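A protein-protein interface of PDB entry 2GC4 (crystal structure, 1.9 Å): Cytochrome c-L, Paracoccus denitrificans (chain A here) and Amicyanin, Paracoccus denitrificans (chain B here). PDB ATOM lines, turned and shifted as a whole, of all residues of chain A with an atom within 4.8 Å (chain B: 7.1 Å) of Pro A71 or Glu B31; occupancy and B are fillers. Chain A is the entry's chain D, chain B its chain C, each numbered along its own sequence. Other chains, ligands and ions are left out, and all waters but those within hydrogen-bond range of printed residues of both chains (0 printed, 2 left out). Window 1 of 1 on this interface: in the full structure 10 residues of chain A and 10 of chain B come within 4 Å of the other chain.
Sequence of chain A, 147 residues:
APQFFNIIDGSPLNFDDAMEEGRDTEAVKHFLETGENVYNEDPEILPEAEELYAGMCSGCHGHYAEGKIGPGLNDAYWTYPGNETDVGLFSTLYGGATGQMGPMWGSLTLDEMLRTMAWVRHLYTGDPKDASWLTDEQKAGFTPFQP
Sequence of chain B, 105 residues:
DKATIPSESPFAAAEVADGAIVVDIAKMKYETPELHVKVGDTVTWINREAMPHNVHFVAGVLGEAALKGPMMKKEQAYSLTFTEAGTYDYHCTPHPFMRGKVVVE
OE1 of Glu B31 lies close to OD1 of Asp A75, 2.7 Å away. The backbone carbonyl oxygen (O) of Glu B31 is in hydrogen-bond range of the backbone NH (N) of Gly A72 (2.9 Å). The side-chain carboxylate (OD1) of Asp A75 lies within salt-bridge range of the side-chain amino group (NZ) of Lys B29, at 2.8 Å. The side-chain hydroxyl (OH) of Tyr A77 is in hydrogen-bond range of the guanidinium group (NE) of Arg B48 (3.3 Å).
N of Tyr A77 sits at hydrogen-bond distance from OD2 of Asp A75, at 2.9 Å. The backbone NH (N) of Glu B31 sits at hydrogen-bond distance from the backbone carbonyl oxygen (O) of Asp B24 (2.9 Å). The backbone carbonyl oxygen of Ile B25 lies within hydrogen-bond range of the backbone NH of Arg B48 (2.8 Å). A ring nitrogen (ND1) of His A61 is in hydrogen-bond range of the backbone carbonyl oxygen of Pro A71, at 2.5 Å. The backbone carbonyl oxygen (O) of His A61 lies within hydrogen-bond range of the backbone NH (N) of Gly A67. OD1 of Asp B24 is in salt-bridge range of NE of Arg B48, 2.8 Å away.
Among the printed residues, pairs that only touch across the chains: Ile A69 with Glu B34 (3.2 Å), Gly A67 with Pro B33 (3.3 Å), Pro A71 with Glu B31 (3.4 Å), Pro A71 with Thr B32 (3.5 Å), Ile A69 with Thr B32 (3.6 Å), Tyr A77 with Asp B24 (3.6 Å), Tyr A77 with Ala B26 (3.7 Å), Asp A75 with Lys B27 (3.8 Å), Gly A70 with Thr B32 (3.98 Å) and Tyr A77 with Glu B31 (3.98 Å).
Printed residues of chain B within 4 Å of Gly A67: Pro B33 (3.3 Å). Printed residues of chain B within 4 Å of Gly A70: Thr B32. Pro A71 touches two residues of chain B. Of the printed residues of chain B, Gly A72 touches Glu B31. Printed residues of chain A within 4 Å of Asp B24: Tyr A77. The nearest residue of chain B that does not touch Pro A71 is Pro B33 (5.7 Å). The nearest printed residue of chain A that does not touch Glu B31 is Gly A67 (4.1 Å).
Printed residues of chain A that touch a printed residue of chain B: Gly A67, Ile A69, Gly A70, Pro A71, Gly A72, Asp A75 and Tyr A77. Of the 15 printed residues of chain B, 9 touch a printed residue of chain A. Hydrophobic or aromatic side chains of chain B that line the printed part of chain A: Ala B26 and Pro B33. Among the printed residues, Asp or Glu carboxylates within 4 Å of a Lys or Arg side-chain nitrogen of the other chain: Asp A75 with Lys B29.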
ATOM      1  N   HIS A  61      28.153 -15.971  -0.776  1.00  0.00           N
ATOM      2  CA  HIS A  61      27.426 -16.739   0.228  1.00  0.00           C
ATOM      3  C   HIS A  61      27.492 -16.209   1.658  1.00  0.00           C
ATOM      4  O   HIS A  61      26.905 -16.794   2.562  1.00  0.00           O
ATOM      5  CB  HIS A  61      27.890 -18.199   0.167  1.00  0.00           C
ATOM      6  CG  HIS A  61      27.441 -18.914  -1.072  1.00  0.00           C
ATOM      7  ND1 HIS A  61      26.124 -19.221  -1.261  1.00  0.00           N
ATOM      8  CD2 HIS A  61      28.348 -19.225  -2.020  1.00  0.00           C
ATOM      9  CE1 HIS A  61      26.176 -19.811  -2.505  1.00  0.00           C
ATOM     10  NE2 HIS A  61      27.521 -19.823  -2.982  1.00  0.00           N
ATOM     11  N   GLU A  66      25.909 -17.654   5.680  1.00  0.00           N
ATOM     12  CA  GLU A  66      24.530 -17.390   6.083  1.00  0.00           C
ATOM     13  C   GLU A  66      23.705 -16.883   4.898  1.00  0.00           C
ATOM     14  O   GLU A  66      22.491 -16.710   5.003  1.00  0.00           O
ATOM     15  CB  GLU A  66      24.493 -16.345   7.210  1.00  0.00           C
ATOM     16  CG  GLU A  66      24.896 -14.929   6.778  1.00  0.00           C
ATOM     17  CD  GLU A  66      26.394 -14.680   6.829  1.00  0.00           C
ATOM     18  OE1 GLU A  66      27.178 -15.564   6.425  1.00  0.00           O
ATOM     19  OE2 GLU A  66      26.793 -13.583   7.267  1.00  0.00           O
ATOM     20  N   GLY A  67      24.369 -16.640   3.771  1.00  0.00           N
ATOM     21  CA  GLY A  67      23.676 -16.145   2.596  1.00  0.00           C
ATOM     22  C   GLY A  67      23.861 -14.647   2.437  1.00  0.00           C
ATOM     23  O   GLY A  67      24.017 -13.928   3.421  1.00  0.00           O
ATOM     24  N   ILE A  69      24.073 -12.358  -1.529  1.00  0.00           N
ATOM     25  CA  ILE A  69      23.423 -12.213  -2.829  1.00  0.00           C
ATOM     26  C   ILE A  69      23.235 -13.619  -3.387  1.00  0.00           C
ATOM     27  O   ILE A  69      22.535 -13.822  -4.374  1.00  0.00           O
ATOM     28  CB  ILE A  69      24.235 -11.335  -3.834  1.00  0.00           C
ATOM     29  CG1 ILE A  69      25.478 -12.071  -4.329  1.00  0.00           C
ATOM     30  CG2 ILE A  69      24.614 -10.019  -3.169  1.00  0.00           C
ATOM     31  CD1 ILE A  69      26.629 -12.005  -3.384  1.00  0.00           C
ATOM     32  N   GLY A  70      23.873 -14.581  -2.727  1.00  0.00           N
ATOM     33  CA  GLY A  70      23.759 -15.982  -3.100  1.00  0.00           C
ATOM     34  C   GLY A  70      23.085 -16.662  -1.916  1.00  0.00           C
ATOM     35  O   GLY A  70      23.037 -16.070  -0.837  1.00  0.00           O
ATOM     36  N   PRO A  71      22.573 -17.893  -2.062  1.00  0.00           N
ATOM     37  CA  PRO A  71      21.901 -18.608  -0.970  1.00  0.00           C
ATOM     38  C   PRO A  71      22.781 -19.082   0.184  1.00  0.00           C
ATOM     39  O   PRO A  71      23.968 -19.371   0.003  1.00  0.00           O
ATOM     40  CB  PRO A  71      21.235 -19.776  -1.690  1.00  0.00           C
ATOM     41  CG  PRO A  71      22.225 -20.091  -2.761  1.00  0.00           C
ATOM     42  CD  PRO A  71      22.577 -18.711  -3.290  1.00  0.00           C
ATOM     43  N   GLY A  72      22.187 -19.163   1.371  1.00  0.00           N
ATOM     44  CA  GLY A  72      22.923 -19.628   2.529  1.00  0.00           C
ATOM     45  C   GLY A  72      23.297 -21.087   2.352  1.00  0.00           C
ATOM     46  O   GLY A  72      22.650 -21.809   1.593  1.00  0.00           O
ATOM     47  N   LEU A  73      24.345 -21.524   3.043  1.00  0.00           N
ATOM     48  CA  LEU A  73      24.801 -22.909   2.952  1.00  0.00           C
ATOM     49  C   LEU A  73      25.017 -23.479   4.348  1.00  0.00           C
ATOM     50  O   LEU A  73      25.665 -24.516   4.494  1.00  0.00           O
ATOM     51  CB  LEU A  73      26.139 -22.980   2.204  1.00  0.00           C
ATOM     52  CG  LEU A  73      26.308 -22.199   0.897  1.00  0.00           C
ATOM     53  CD1 LEU A  73      27.781 -22.206   0.501  1.00  0.00           C
ATOM     54  CD2 LEU A  73      25.446 -22.806  -0.192  1.00  0.00           C
ATOM     55  N   ASP A  75      22.526 -24.402   6.810  1.00  0.00           N
ATOM     56  CA  ASP A  75      21.444 -25.109   7.485  1.00  0.00           C
ATOM     57  C   ASP A  75      21.083 -26.384   6.736  1.00  0.00           C
ATOM     58  O   ASP A  75      21.690 -26.696   5.713  1.00  0.00           O
ATOM     59  CB  ASP A  75      20.220 -24.193   7.673  1.00  0.00           C
ATOM     60  CG  ASP A  75      19.583 -23.762   6.364  1.00  0.00           C
ATOM     61  OD1 ASP A  75      18.931 -22.695   6.364  1.00  0.00           O
ATOM     62  OD2 ASP A  75      19.709 -24.483   5.349  1.00  0.00           O
ATOM     63  N   TYR A  77      18.674 -27.126   4.809  1.00  0.00           N
ATOM     64  CA  TYR A  77      17.992 -27.044   3.523  1.00  0.00           C
ATOM     65  C   TYR A  77      18.974 -26.904   2.364  1.00  0.00           C
ATOM     66  O   TYR A  77      19.923 -26.118   2.431  1.00  0.00           O
ATOM     67  CB  TYR A  77      17.013 -25.861   3.475  1.00  0.00           C
ATOM     68  CG  TYR A  77      16.387 -25.718   2.105  1.00  0.00           C
ATOM     69  CD1 TYR A  77      15.411 -26.617   1.671  1.00  0.00           C
ATOM     70  CD2 TYR A  77      16.844 -24.756   1.204  1.00  0.00           C
ATOM     71  CE1 TYR A  77      14.911 -26.571   0.371  1.00  0.00           C
ATOM     72  CE2 TYR A  77      16.350 -24.700  -0.102  1.00  0.00           C
ATOM     73  CZ  TYR A  77      15.386 -25.615  -0.508  1.00  0.00           C
ATOM     74  OH  TYR A  77      14.912 -25.592  -1.798  1.00  0.00           O
ATOM     75  N   VAL B  22      14.523 -17.178  -7.974  1.00  0.00           N
ATOM     76  CA  VAL B  22      13.836 -17.744  -6.820  1.00  0.00           C
ATOM     77  C   VAL B  22      14.512 -17.517  -5.471  1.00  0.00           C
ATOM     78  O   VAL B  22      15.731 -17.609  -5.350  1.00  0.00           O
ATOM     79  CB  VAL B  22      13.647 -19.277  -7.005  1.00  0.00           C
ATOM     80  CG1 VAL B  22      13.186 -19.922  -5.703  1.00  0.00           C
ATOM     81  CG2 VAL B  22      12.636 -19.548  -8.115  1.00  0.00           C
ATOM     82  N   VAL B  23      13.701 -17.215  -4.460  1.00  0.00           N
ATOM     83  CA  VAL B  23      14.193 -17.034  -3.098  1.00  0.00           C
ATOM     84  C   VAL B  23      13.490 -18.114  -2.285  1.00  0.00           C
ATOM     85  O   VAL B  23      12.271 -18.065  -2.107  1.00  0.00           O
ATOM     86  CB  VAL B  23      13.824 -15.649  -2.514  1.00  0.00           C
ATOM     87  CG1 VAL B  23      14.187 -15.594  -1.027  1.00  0.00           C
ATOM     88  CG2 VAL B  23      14.564 -14.551  -3.268  1.00  0.00           C
ATOM     89  N   ASP B  24      14.248 -19.097  -1.812  1.00  0.00           N
ATOM     90  CA  ASP B  24      13.674 -20.184  -1.027  1.00  0.00           C
ATOM     91  C   ASP B  24      13.483 -19.767   0.421  1.00  0.00           C
ATOM     92  O   ASP B  24      14.286 -19.020   0.976  1.00  0.00           O
ATOM     93  CB  ASP B  24      14.575 -21.424  -1.051  1.00  0.00           C
ATOM     94  CG  ASP B  24      14.719 -22.022  -2.436  1.00  0.00           C
ATOM     95  OD1 ASP B  24      13.688 -22.402  -3.034  1.00  0.00           O
ATOM     96  OD2 ASP B  24      15.869 -22.112  -2.918  1.00  0.00           O
ATOM     97  N   ILE B  25      12.412 -20.262   1.025  1.00  0.00           N
ATOM     98  CA  ILE B  25      12.128 -19.970   2.418  1.00  0.00           C
ATOM     99  C   ILE B  25      12.201 -21.295   3.159  1.00  0.00           C
ATOM    100  O   ILE B  25      11.457 -22.227   2.848  1.00  0.00           O
ATOM    101  CB  ILE B  25      10.716 -19.379   2.600  1.00  0.00           C
ATOM    102  CG1 ILE B  25      10.547 -18.143   1.716  1.00  0.00           C
ATOM    103  CG2 ILE B  25      10.501 -18.990   4.058  1.00  0.00           C
ATOM    104  CD1 ILE B  25       9.158 -17.530   1.796  1.00  0.00           C
ATOM    105  N   ALA B  26      13.113 -21.390   4.119  1.00  0.00           N
ATOM    106  CA  ALA B  26      13.256 -22.616   4.900  1.00  0.00           C
ATOM    107  C   ALA B  26      13.961 -22.329   6.217  1.00  0.00           C
ATOM    108  O   ALA B  26      14.734 -21.373   6.326  1.00  0.00           O
ATOM    109  CB  ALA B  26      14.037 -23.660   4.106  1.00  0.00           C
ATOM    110  N   LYS B  27      13.682 -23.156   7.217  1.00  0.00           N
ATOM    111  CA  LYS B  27      14.299 -23.002   8.524  1.00  0.00           C
ATOM    112  C   LYS B  27      14.158 -21.585   9.070  1.00  0.00           C
ATOM    113  O   LYS B  27      15.118 -21.003   9.579  1.00  0.00           O
ATOM    114  CB  LYS B  27      15.778 -23.395   8.445  1.00  0.00           C
ATOM    115  CG  LYS B  27      16.004 -24.831   7.974  1.00  0.00           C
ATOM    116  CD  LYS B  27      15.387 -25.821   8.949  1.00  0.00           C
ATOM    117  CE  LYS B  27      15.489 -27.245   8.438  1.00  0.00           C
ATOM    118  NZ  LYS B  27      14.916 -28.227   9.403  1.00  0.00           N
ATOM    119  N   MET B  28      12.957 -21.032   8.944  1.00  0.00           N
ATOM    120  CA  MET B  28      12.654 -19.695   9.446  1.00  0.00           C
ATOM    121  C   MET B  28      13.497 -18.580   8.847  1.00  0.00           C
ATOM    122  O   MET B  28      13.833 -17.617   9.539  1.00  0.00           O
ATOM    123  CB  MET B  28      12.804 -19.658  10.972  1.00  0.00           C
ATOM    124  CG  MET B  28      11.950 -20.667  11.710  1.00  0.00           C
ATOM    125  SD  MET B  28      10.198 -20.435  11.395  1.00  0.00           S
ATOM    126  CE  MET B  28       9.831 -19.102  12.515  1.00  0.00           C
ATOM    127  N   LYS B  29      13.841 -18.689   7.569  1.00  0.00           N
ATOM    128  CA  LYS B  29      14.639 -17.638   6.948  1.00  0.00           C
ATOM    129  C   LYS B  29      14.510 -17.578   5.434  1.00  0.00           C
ATOM    130  O   LYS B  29      14.162 -18.563   4.783  1.00  0.00           O
ATOM    131  CB  LYS B  29      16.124 -17.813   7.304  1.00  0.00           C
ATOM    132  CG  LYS B  29      16.832 -18.906   6.516  1.00  0.00           C
ATOM    133  CD  LYS B  29      18.343 -18.899   6.750  1.00  0.00           C
ATOM    134  CE  LYS B  29      18.701 -19.423   8.130  1.00  0.00           C
ATOM    135  NZ  LYS B  29      18.263 -20.836   8.304  1.00  0.00           N
ATOM    136  N   TYR B  30      14.775 -16.398   4.884  1.00  0.00           N
ATOM    137  CA  TYR B  30      14.765 -16.208   3.441  1.00  0.00           C
ATOM    138  C   TYR B  30      16.208 -16.587   3.113  1.00  0.00           C
ATOM    139  O   TYR B  30      17.138 -15.876   3.497  1.00  0.00           O
ATOM    140  CB  TYR B  30      14.478 -14.744   3.106  1.00  0.00           C
ATOM    141  CG  TYR B  30      13.098 -14.300   3.548  1.00  0.00           C
ATOM    142  CD1 TYR B  30      11.950 -14.842   2.966  1.00  0.00           C
ATOM    143  CD2 TYR B  30      12.938 -13.354   4.564  1.00  0.00           C
ATOM    144  CE1 TYR B  30      10.670 -14.455   3.385  1.00  0.00           C
ATOM    145  CE2 TYR B  30      11.660 -12.958   4.992  1.00  0.00           C
ATOM    146  CZ  TYR B  30      10.535 -13.511   4.399  1.00  0.00           C
ATOM    147  OH  TYR B  30       9.279 -13.114   4.811  1.00  0.00           O
ATOM    148  N   GLU B  31      16.389 -17.717   2.433  1.00  0.00           N
ATOM    149  CA  GLU B  31      17.728 -18.222   2.124  1.00  0.00           C
ATOM    150  C   GLU B  31      18.672 -17.277   1.383  1.00  0.00           C
ATOM    151  O   GLU B  31      19.891 -17.406   1.497  1.00  0.00           O
ATOM    152  CB  GLU B  31      17.624 -19.565   1.400  1.00  0.00           C
ATOM    153  CG  GLU B  31      17.028 -20.686   2.263  1.00  0.00           C
ATOM    154  CD  GLU B  31      17.898 -21.068   3.466  1.00  0.00           C
ATOM    155  OE1 GLU B  31      17.505 -21.980   4.222  1.00  0.00           O
ATOM    156  OE2 GLU B  31      18.976 -20.468   3.660  1.00  0.00           O
ATOM    157  N   THR B  32      18.125 -16.337   0.620  1.00  0.00           N
ATOM    158  CA  THR B  32      18.956 -15.352  -0.066  1.00  0.00           C
ATOM    159  C   THR B  32      18.466 -14.010   0.476  1.00  0.00           C
ATOM    160  O   THR B  32      17.539 -13.412  -0.062  1.00  0.00           O
ATOM    161  CB  THR B  32      18.779 -15.407  -1.600  1.00  0.00           C
ATOM    162  OG1 THR B  32      19.111 -16.717  -2.079  1.00  0.00           O
ATOM    163  CG2 THR B  32      19.701 -14.395  -2.272  1.00  0.00           C
ATOM    164  N   PRO B  33      19.089 -13.530   1.561  1.00  0.00           N
ATOM    165  CA  PRO B  33      18.777 -12.276   2.256  1.00  0.00           C
ATOM    166  C   PRO B  33      18.912 -10.960   1.487  1.00  0.00           C
ATOM    167  O   PRO B  33      18.163 -10.015   1.742  1.00  0.00           O
ATOM    168  CB  PRO B  33      19.696 -12.332   3.473  1.00  0.00           C
ATOM    169  CG  PRO B  33      20.896 -13.028   2.933  1.00  0.00           C
ATOM    170  CD  PRO B  33      20.275 -14.167   2.161  1.00  0.00           C
ATOM    171  N   GLU B  34      19.866 -10.885   0.566  1.00  0.00           N
ATOM    172  CA  GLU B  34      20.062  -9.663  -0.211  1.00  0.00           C
ATOM    173  C   GLU B  34      20.111  -9.978  -1.702  1.00  0.00           C
ATOM    174  O   GLU B  34      21.184 -10.047  -2.303  1.00  0.00           O
ATOM    175  CB  GLU B  34      21.354  -8.962   0.211  1.00  0.00           C
ATOM    176  CG  GLU B  34      21.546  -7.609  -0.453  1.00  0.00           C
ATOM    177  CD  GLU B  34      22.880  -6.970  -0.116  1.00  0.00           C
ATOM    178  OE1 GLU B  34      23.189  -6.830   1.087  1.00  0.00           O
ATOM    179  OE2 GLU B  34      23.617  -6.601  -1.057  1.00  0.00           O
ATOM    180  N   ARG B  48       9.619 -23.714   1.443  1.00  0.00           N
ATOM    181  CA  ARG B  48      10.086 -25.094   1.392  1.00  0.00           C
ATOM    182  C   ARG B  48       9.778 -25.908   2.644  1.00  0.00           C
ATOM    183  O   ARG B  48      10.167 -27.073   2.735  1.00  0.00           O
ATOM    184  CB  ARG B  48      11.596 -25.117   1.146  1.00  0.00           C
ATOM    185  CG  ARG B  48      12.021 -24.448  -0.147  1.00  0.00           C
ATOM    186  CD  ARG B  48      11.489 -25.195  -1.360  1.00  0.00           C
ATOM    187  NE  ARG B  48      11.922 -24.559  -2.600  1.00  0.00           N
ATOM    188  CZ  ARG B  48      11.675 -25.038  -3.813  1.00  0.00           C
ATOM    189  NH1 ARG B  48      12.109 -24.387  -4.883  1.00  0.00           N
ATOM    190  NH2 ARG B  48      10.999 -26.168  -3.954  1.00  0.00           N
ATOM    191  N   TYR B  90      11.619  -6.210   3.380  1.00  0.00           N
ATOM    192  CA  TYR B  90      10.384  -6.911   3.676  1.00  0.00           C
ATOM    193  C   TYR B  90      10.616  -7.862   4.842  1.00  0.00           C
ATOM    194  O   TYR B  90      11.762  -8.099   5.244  1.00  0.00           O
ATOM    195  CB  TYR B  90       9.888  -7.694   2.449  1.00  0.00           C
ATOM    196  CG  TYR B  90      10.820  -8.792   1.975  1.00  0.00           C
ATOM    197  CD1 TYR B  90      11.870  -8.517   1.097  1.00  0.00           C
ATOM    198  CD2 TYR B  90      10.655 -10.107   2.412  1.00  0.00           C
ATOM    199  CE1 TYR B  90      12.735  -9.529   0.660  1.00  0.00           C
ATOM    200  CE2 TYR B  90      11.513 -11.125   1.987  1.00  0.00           C
ATOM    201  CZ  TYR B  90      12.550 -10.830   1.112  1.00  0.00           C
ATOM    202  OH  TYR B  90      13.398 -11.835   0.693  1.00  0.00           O
